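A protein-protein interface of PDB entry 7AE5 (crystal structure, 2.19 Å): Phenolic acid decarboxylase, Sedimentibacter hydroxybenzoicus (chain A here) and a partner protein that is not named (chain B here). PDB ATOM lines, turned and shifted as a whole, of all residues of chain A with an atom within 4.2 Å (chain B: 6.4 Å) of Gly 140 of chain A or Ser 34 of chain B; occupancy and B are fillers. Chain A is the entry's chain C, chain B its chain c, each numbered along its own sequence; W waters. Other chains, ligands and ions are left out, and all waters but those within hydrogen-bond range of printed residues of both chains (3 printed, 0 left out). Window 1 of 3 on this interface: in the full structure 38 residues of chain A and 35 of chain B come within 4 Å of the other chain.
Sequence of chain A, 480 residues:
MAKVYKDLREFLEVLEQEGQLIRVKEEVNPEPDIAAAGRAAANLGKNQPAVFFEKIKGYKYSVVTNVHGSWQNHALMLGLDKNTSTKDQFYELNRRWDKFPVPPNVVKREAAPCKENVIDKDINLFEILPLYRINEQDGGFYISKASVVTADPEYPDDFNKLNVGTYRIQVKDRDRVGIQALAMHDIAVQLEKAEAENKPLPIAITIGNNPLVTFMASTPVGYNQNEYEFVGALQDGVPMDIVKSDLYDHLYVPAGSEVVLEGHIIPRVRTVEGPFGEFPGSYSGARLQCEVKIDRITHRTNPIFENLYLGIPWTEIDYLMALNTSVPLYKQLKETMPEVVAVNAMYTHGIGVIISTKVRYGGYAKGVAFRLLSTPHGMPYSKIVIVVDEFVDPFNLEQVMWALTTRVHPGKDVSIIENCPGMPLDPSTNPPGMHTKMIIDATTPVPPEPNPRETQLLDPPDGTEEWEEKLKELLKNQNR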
ATOM      1  N   ARG A 133     -26.026  19.117 -20.785  1.00  0.00           N
ATOM      2  CA  ARG A 133     -25.540  18.677 -19.484  1.00  0.00           C
ATOM      3  C   ARG A 133     -26.314  17.435 -19.059  1.00  0.00           C
ATOM      4  O   ARG A 133     -27.549  17.452 -19.008  1.00  0.00           O
ATOM      5  CB  ARG A 133     -25.671  19.778 -18.433  1.00  0.00           C
ATOM      6  CG  ARG A 133     -24.846  19.497 -17.183  1.00  0.00           C
ATOM      7  CD  ARG A 133     -25.024  20.562 -16.115  1.00  0.00           C
ATOM      8  NE  ARG A 133     -24.845  21.908 -16.643  1.00  0.00           N
ATOM      9  CZ  ARG A 133     -23.670  22.509 -16.775  1.00  0.00           C
ATOM     10  NH1 ARG A 133     -22.543  21.903 -16.441  1.00  0.00           N
ATOM     11  NH2 ARG A 133     -23.627  23.747 -17.251  1.00  0.00           N
ATOM     12  N   ASP A 138     -22.434  18.154 -13.261  1.00  0.00           N
ATOM     13  CA  ASP A 138     -21.335  17.947 -14.192  1.00  0.00           C
ATOM     14  C   ASP A 138     -20.587  19.255 -14.431  1.00  0.00           C
ATOM     15  O   ASP A 138     -21.166  20.344 -14.392  1.00  0.00           O
ATOM     16  CB  ASP A 138     -21.853  17.389 -15.519  1.00  0.00           C
ATOM     17  CG  ASP A 138     -22.287  15.936 -15.412  1.00  0.00           C
ATOM     18  OD1 ASP A 138     -21.750  15.217 -14.544  1.00  0.00           O
ATOM     19  OD2 ASP A 138     -23.156  15.511 -16.206  1.00  0.00           O
ATOM     20  N   GLY A 139     -19.279  19.138 -14.676  1.00  0.00           N
ATOM     21  CA  GLY A 139     -18.453  20.304 -14.942  1.00  0.00           C
ATOM     22  C   GLY A 139     -18.740  20.981 -16.267  1.00  0.00           C
ATOM     23  O   GLY A 139     -18.507  22.187 -16.399  1.00  0.00           O
ATOM     24  N   GLY A 140     -19.232  20.238 -17.244  1.00  0.00           N
ATOM     25  CA  GLY A 140     -19.602  20.809 -18.518  1.00  0.00           C
ATOM     26  C   GLY A 140     -20.518  19.872 -19.269  1.00  0.00           C
ATOM     27  O   GLY A 140     -21.111  18.958 -18.694  1.00  0.00           O
ATOM     28  N   PHE A 141     -20.639  20.110 -20.573  1.00  0.00           N
ATOM     29  CA  PHE A 141     -21.365  19.189 -21.435  1.00  0.00           C
ATOM     30  C   PHE A 141     -20.448  18.036 -21.823  1.00  0.00           C
ATOM     31  O   PHE A 141     -19.276  18.243 -22.151  1.00  0.00           O
ATOM     32  CB  PHE A 141     -21.883  19.902 -22.684  1.00  0.00           C
ATOM     33  CG  PHE A 141     -22.600  21.194 -22.397  1.00  0.00           C
ATOM     34  CD1 PHE A 141     -23.392  21.333 -21.267  1.00  0.00           C
ATOM     35  CD2 PHE A 141     -22.483  22.267 -23.263  1.00  0.00           C
ATOM     36  CE1 PHE A 141     -24.050  22.521 -21.006  1.00  0.00           C
ATOM     37  CE2 PHE A 141     -23.140  23.457 -23.009  1.00  0.00           C
ATOM     38  CZ  PHE A 141     -23.923  23.585 -21.878  1.00  0.00           C
ATOM     39  N   TYR A 142     -20.982  16.819 -21.779  1.00  0.00           N
ATOM     40  CA  TYR A 142     -20.172  15.619 -21.916  1.00  0.00           C
ATOM     41  C   TYR A 142     -20.608  14.791 -23.117  1.00  0.00           C
ATOM     42  O   TYR A 142     -21.803  14.678 -23.411  1.00  0.00           O
ATOM     43  CB  TYR A 142     -20.253  14.763 -20.649  1.00  0.00           C
ATOM     44  CG  TYR A 142     -19.149  15.024 -19.649  1.00  0.00           C
ATOM     45  CD1 TYR A 142     -19.224  16.091 -18.763  1.00  0.00           C
ATOM     46  CD2 TYR A 142     -18.036  14.199 -19.585  1.00  0.00           C
ATOM     47  CE1 TYR A 142     -18.218  16.331 -17.842  1.00  0.00           C
ATOM     48  CE2 TYR A 142     -17.026  14.428 -18.670  1.00  0.00           C
ATOM     49  CZ  TYR A 142     -17.123  15.493 -17.799  1.00  0.00           C
ATOM     50  OH  TYR A 142     -16.116  15.721 -16.893  1.00  0.00           O
ATOM     51  N   GLN A 170     -15.332  15.503 -21.811  1.00  0.00           N
ATOM     52  CA  GLN A 170     -15.911  16.788 -21.441  1.00  0.00           C
ATOM     53  C   GLN A 170     -15.570  17.837 -22.486  1.00  0.00           C
ATOM     54  O   GLN A 170     -14.399  18.031 -22.823  1.00  0.00           O
ATOM     55  CB  GLN A 170     -15.408  17.248 -20.073  1.00  0.00           C
ATOM     56  CG  GLN A 170     -15.996  18.590 -19.652  1.00  0.00           C
ATOM     57  CD  GLN A 170     -15.459  19.087 -18.323  1.00  0.00           C
ATOM     58  OE1 GLN A 170     -14.809  18.347 -17.587  1.00  0.00           O
ATOM     59  NE2 GLN A 170     -15.732  20.351 -18.009  1.00  0.00           N
ATOM     60  N   ARG B   5     -19.190  28.108 -10.179  1.00  0.00           N
ATOM     61  CA  ARG B   5     -18.435  27.120  -9.418  1.00  0.00           C
ATOM     62  C   ARG B   5     -17.335  27.754  -8.570  1.00  0.00           C
ATOM     63  O   ARG B   5     -17.222  27.460  -7.377  1.00  0.00           O
ATOM     64  CB  ARG B   5     -17.833  26.079 -10.365  1.00  0.00           C
ATOM     65  CG  ARG B   5     -16.817  25.162  -9.709  1.00  0.00           C
ATOM     66  CD  ARG B   5     -16.795  23.805 -10.385  1.00  0.00           C
ATOM     67  NE  ARG B   5     -15.893  23.780 -11.530  1.00  0.00           N
ATOM     68  CZ  ARG B   5     -15.723  22.732 -12.324  1.00  0.00           C
ATOM     69  NH1 ARG B   5     -16.389  21.605 -12.132  1.00  0.00           N
ATOM     70  NH2 ARG B   5     -14.867  22.818 -13.338  1.00  0.00           N
ATOM     71  N   MET B  14     -18.302  30.921 -25.065  1.00  0.00           N
ATOM     72  CA  MET B  14     -17.779  29.825 -25.871  1.00  0.00           C
ATOM     73  C   MET B  14     -18.403  29.818 -27.262  1.00  0.00           C
ATOM     74  O   MET B  14     -17.696  29.907 -28.271  1.00  0.00           O
ATOM     75  CB  MET B  14     -18.026  28.491 -25.162  1.00  0.00           C
ATOM     76  CG  MET B  14     -16.974  27.434 -25.441  1.00  0.00           C
ATOM     77  SD  MET B  14     -17.597  25.775 -25.119  1.00  0.00           S
ATOM     78  CE  MET B  14     -17.467  25.717 -23.335  1.00  0.00           C
ATOM     79  N   VAL B  25     -23.386  29.804 -24.645  1.00  0.00           N
ATOM     80  CA  VAL B  25     -22.669  28.970 -23.687  1.00  0.00           C
ATOM     81  C   VAL B  25     -21.448  29.734 -23.203  1.00  0.00           C
ATOM     82  O   VAL B  25     -20.653  30.223 -24.015  1.00  0.00           O
ATOM     83  CB  VAL B  25     -22.261  27.614 -24.290  1.00  0.00           C
ATOM     84  CG1 VAL B  25     -21.632  26.738 -23.221  1.00  0.00           C
ATOM     85  CG2 VAL B  25     -23.466  26.921 -24.901  1.00  0.00           C
ATOM     86  N   TYR B  26     -21.299  29.832 -21.887  1.00  0.00           N
ATOM     87  CA  TYR B  26     -20.177  30.509 -21.258  1.00  0.00           C
ATOM     88  C   TYR B  26     -19.254  29.483 -20.618  1.00  0.00           C
ATOM     89  O   TYR B  26     -19.668  28.371 -20.285  1.00  0.00           O
ATOM     90  CB  TYR B  26     -20.668  31.514 -20.213  1.00  0.00           C
ATOM     91  CG  TYR B  26     -21.708  32.463 -20.759  1.00  0.00           C
ATOM     92  CD1 TYR B  26     -21.345  33.522 -21.577  1.00  0.00           C
ATOM     93  CD2 TYR B  26     -23.056  32.285 -20.475  1.00  0.00           C
ATOM     94  CE1 TYR B  26     -22.292  34.388 -22.087  1.00  0.00           C
ATOM     95  CE2 TYR B  26     -24.011  33.146 -20.980  1.00  0.00           C
ATOM     96  CZ  TYR B  26     -23.624  34.194 -21.786  1.00  0.00           C
ATOM     97  OH  TYR B  26     -24.571  35.053 -22.291  1.00  0.00           O
ATOM     98  N   VAL B  27     -17.988  29.863 -20.458  1.00  0.00           N
ATOM     99  CA  VAL B  27     -16.979  28.985 -19.875  1.00  0.00           C
ATOM    100  C   VAL B  27     -16.027  29.816 -19.026  1.00  0.00           C
ATOM    101  O   VAL B  27     -15.604  30.907 -19.426  1.00  0.00           O
ATOM    102  CB  VAL B  27     -16.214  28.188 -20.958  1.00  0.00           C
ATOM    103  CG1 VAL B  27     -15.573  29.125 -21.977  1.00  0.00           C
ATOM    104  CG2 VAL B  27     -15.172  27.269 -20.321  1.00  0.00           C
ATOM    105  N   CYS B  28     -15.706  29.301 -17.844  1.00  0.00           N
ATOM    106  CA  CYS B  28     -14.763  29.953 -16.950  1.00  0.00           C
ATOM    107  C   CYS B  28     -13.338  29.659 -17.398  1.00  0.00           C
ATOM    108  O   CYS B  28     -12.993  28.508 -17.681  1.00  0.00           O
ATOM    109  CB  CYS B  28     -14.983  29.474 -15.516  1.00  0.00           C
ATOM    110  SG  CYS B  28     -13.742  30.026 -14.338  1.00  0.00           S
ATOM    111  N   CYS B  32     -12.616  26.064 -15.937  1.00  0.00           N
ATOM    112  CA  CYS B  32     -13.173  25.396 -17.112  1.00  0.00           C
ATOM    113  C   CYS B  32     -14.645  25.029 -16.971  1.00  0.00           C
ATOM    114  O   CYS B  32     -15.177  24.322 -17.835  1.00  0.00           O
ATOM    115  CB  CYS B  32     -12.381  24.136 -17.483  1.00  0.00           C
ATOM    116  SG  CYS B  32     -10.590  24.344 -17.479  1.00  0.00           S
ATOM    117  N   TYR B  33     -15.321  25.481 -15.917  1.00  0.00           N
ATOM    118  CA  TYR B  33     -16.755  25.248 -15.807  1.00  0.00           C
ATOM    119  C   TYR B  33     -17.488  25.976 -16.928  1.00  0.00           C
ATOM    120  O   TYR B  33     -17.192  27.132 -17.236  1.00  0.00           O
ATOM    121  CB  TYR B  33     -17.273  25.720 -14.447  1.00  0.00           C
ATOM    122  CG  TYR B  33     -18.712  25.341 -14.167  1.00  0.00           C
ATOM    123  CD1 TYR B  33     -19.069  24.023 -13.907  1.00  0.00           C
ATOM    124  CD2 TYR B  33     -19.714  26.303 -14.157  1.00  0.00           C
ATOM    125  CE1 TYR B  33     -20.385  23.675 -13.647  1.00  0.00           C
ATOM    126  CE2 TYR B  33     -21.032  25.965 -13.900  1.00  0.00           C
ATOM    127  CZ  TYR B  33     -21.361  24.650 -13.645  1.00  0.00           C
ATOM    128  OH  TYR B  33     -22.670  24.311 -13.389  1.00  0.00           O
ATOM    129  N   SER B  34     -18.444  25.288 -17.545  1.00  0.00           N
ATOM    130  CA  SER B  34     -19.211  25.851 -18.645  1.00  0.00           C
ATOM    131  C   SER B  34     -20.699  25.647 -18.399  1.00  0.00           C
ATOM    132  O   SER B  34     -21.106  24.710 -17.704  1.00  0.00           O
ATOM    133  CB  SER B  34     -18.812  25.230 -19.990  1.00  0.00           C
ATOM    134  OG  SER B  34     -19.114  23.848 -20.023  1.00  0.00           O
ATOM    135  N   TRP B  35     -21.508  26.532 -18.978  1.00  0.00           N
ATOM    136  CA  TRP B  35     -22.949  26.470 -18.775  1.00  0.00           C
ATOM    137  C   TRP B  35     -23.661  27.270 -19.856  1.00  0.00           C
ATOM    138  O   TRP B  35     -23.097  28.193 -20.450  1.00  0.00           O
ATOM    139  CB  TRP B  35     -23.340  26.977 -17.381  1.00  0.00           C
ATOM    140  CG  TRP B  35     -23.163  28.453 -17.182  1.00  0.00           C
ATOM    141  CD1 TRP B  35     -24.109  29.424 -17.348  1.00  0.00           C
ATOM    142  CD2 TRP B  35     -21.969  29.125 -16.764  1.00  0.00           C
ATOM    143  NE1 TRP B  35     -23.576  30.657 -17.064  1.00  0.00           N
ATOM    144  CE2 TRP B  35     -22.264  30.502 -16.704  1.00  0.00           C
ATOM    145  CE3 TRP B  35     -20.678  28.698 -16.440  1.00  0.00           C
ATOM    146  CZ2 TRP B  35     -21.315  31.453 -16.331  1.00  0.00           C
ATOM    147  CZ3 TRP B  35     -19.738  29.642 -16.069  1.00  0.00           C
ATOM    148  CH2 TRP B  35     -20.062  31.004 -16.017  1.00  0.00           C
ATOM    149  N   ARG B  36     -24.914  26.896 -20.095  1.00  0.00           N
ATOM    150  CA  ARG B  36     -25.772  27.572 -21.055  1.00  0.00           C
ATOM    151  C   ARG B  36     -26.503  28.728 -20.385  1.00  0.00           C
ATOM    152  O   ARG B  36     -26.832  28.673 -19.196  1.00  0.00           O
ATOM    153  CB  ARG B  36     -26.786  26.591 -21.650  1.00  0.00           C
ATOM    154  CG  ARG B  36     -27.158  26.862 -23.099  1.00  0.00           C
ATOM    155  CD  ARG B  36     -28.190  25.857 -23.595  1.00  0.00           C
ATOM    156  NE  ARG B  36     -27.766  24.479 -23.373  1.00  0.00           N
ATOM    157  CZ  ARG B  36     -26.968  23.801 -24.187  1.00  0.00           C
ATOM    158  NH1 ARG B  36     -26.483  24.344 -25.290  1.00  0.00           N
ATOM    159  NH2 ARG B  36     -26.648  22.546 -23.884  1.00  0.00           N
ATOM    160  N   GLU B  39     -29.584  27.824 -18.470  1.00  0.00           N
ATOM    161  CA  GLU B  39     -29.457  27.202 -17.163  1.00  0.00           C
ATOM    162  C   GLU B  39     -29.346  28.261 -16.070  1.00  0.00           C
ATOM    163  O   GLU B  39     -28.988  29.415 -16.315  1.00  0.00           O
ATOM    164  CB  GLU B  39     -28.230  26.290 -17.108  1.00  0.00           C
ATOM    165  CG  GLU B  39     -28.361  24.980 -17.860  1.00  0.00           C
ATOM    166  CD  GLU B  39     -27.196  24.044 -17.586  1.00  0.00           C
ATOM    167  OE1 GLU B  39     -26.181  24.134 -18.309  1.00  0.00           O
ATOM    168  OE2 GLU B  39     -27.295  23.218 -16.651  1.00  0.00           O
ATOM    169  N   PRO B  41     -27.432  27.503 -12.854  1.00  0.00           N
ATOM    170  CA  PRO B  41     -26.759  26.416 -12.127  1.00  0.00           C
ATOM    171  C   PRO B  41     -26.572  26.743 -10.652  1.00  0.00           C
ATOM    172  O   PRO B  41     -26.085  27.818 -10.293  1.00  0.00           O
ATOM    173  CB  PRO B  41     -25.410  26.285 -12.848  1.00  0.00           C
ATOM    174  CG  PRO B  41     -25.548  27.082 -14.119  1.00  0.00           C
ATOM    175  CD  PRO B  41     -26.530  28.162 -13.811  1.00  0.00           C
HETATM  176  O   HOH W   1     -16.824  22.619 -19.313  1.00  0.00           O
HETATM  177  O   HOH W   2     -19.234  21.911 -22.045  1.00  0.00           O
HETATM  178  O   HOH W   3     -23.077  21.615 -13.028  1.00  0.00           O
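Water W3 lies within hydrogen-bond range of the backbone carbonyl oxygen (O) of Asp 138 of chain A (2.7 Å), the side-chain hydroxyl (OH) of Tyr 33 of chain B (2.8 Å) and the guanidinium group (NH1) of Arg 133 of chain A (3.5 Å). Water W1 lies within hydrogen-bond range of OG of Ser 34 of chain B (2.7 Å), O of Cys 32 of chain B (2.8 Å), NE2 of Gln 170 of chain A (2.8 Å) and O of Gly 139 of chain A (3.4 Å). Water W2 bridges N of Phe 141 of chain A and OG of Ser 34 of chain B.
O of Ser 34 of chain B is in hydrogen-bond range of NH2 of Arg 133 of chain A, at 2.7 Å. The side-chain carboxylate (OE2) of Glu 39 of chain B lies within salt-bridge range of the guanidinium group (NE) of Arg 133 of chain A (2.8 Å). The backbone carbonyl oxygen (O) of Gly 139 of chain A is in hydrogen-bond range of the backbone NH (N) of Ser 34 of chain B, 3.3 Å away.
Of the printed residues of chain B, Asp 138 of chain A touches Tyr 33 (3.5 Å). Gly 140 of chain A touches one residue of chain B. Of the printed residues of chain A, Arg 5 of chain B touches Gly 139 (3.7 Å). Of the printed residues of chain A, Val 25 of chain B touches Phe 141. Cys 32 of chain B touches none of the printed residues of chain A. Of the printed residues of chain A, Tyr 33 of chain B touches Arg 133, Asp 138 and Gly 139. The nearest residue of chain B that does not touch Gly 140 of chain A is Tyr 33 of chain B (5.0 Å). The nearest residue of chain A that does not touch Ser 34 of chain B is Phe 141 of chain A (4.1 Å).
Hydrophobic or aromatic side chains of chain A that line the printed part of chain B: Phe 141. Along chain A the printed residues that touch a printed residue of chain B span positions 133 to 141. Among the printed residues, 12 pairs touch across the chains. Among the printed residues, Asp or Glu carboxylates within 4 Å of a Lys or Arg side-chain nitrogen of the other chain: Arg 133 of chain A with Glu 39 of chain B.
The guanidinium group (NH1) of Arg 133 of chain A sits at hydrogen-bond distance from the backbone carbonyl oxygen (O) of Asp 138 of chain A (2.9 Å). O of Val 25 of chain B is in hydrogen-bond range of N of Met 14 of chain B (2.7 Å). N of Tyr 26 of chain B lies within hydrogen-bond range of O of Trp 35 of chain B (2.8 Å). The backbone carbonyl oxygen (O) of Tyr 33 of chain B sits at hydrogen-bond distance from the backbone NH (N) of Cys 28 of chain B (2.7 Å).
Among the printed residues, pairs that only touch across the chains: Arg 133 of chain A with Tyr 33 of chain B, Arg 133 of chain A with Trp 35 of chain B, Asp 138 of chain A with Tyr 33 of chain B, Gly 139 of chain A with Arg 5 of chain B, Gly 139 of chain A with Tyr 33 of chain B, Gly 140 of chain A with Ser 34 of chain B, Phe 141 of chain A with Val 25 of chain B, Phe 141 of chain A with Arg 36 of chain B and Phe 141 of chain A with Glu 39 of chain B.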
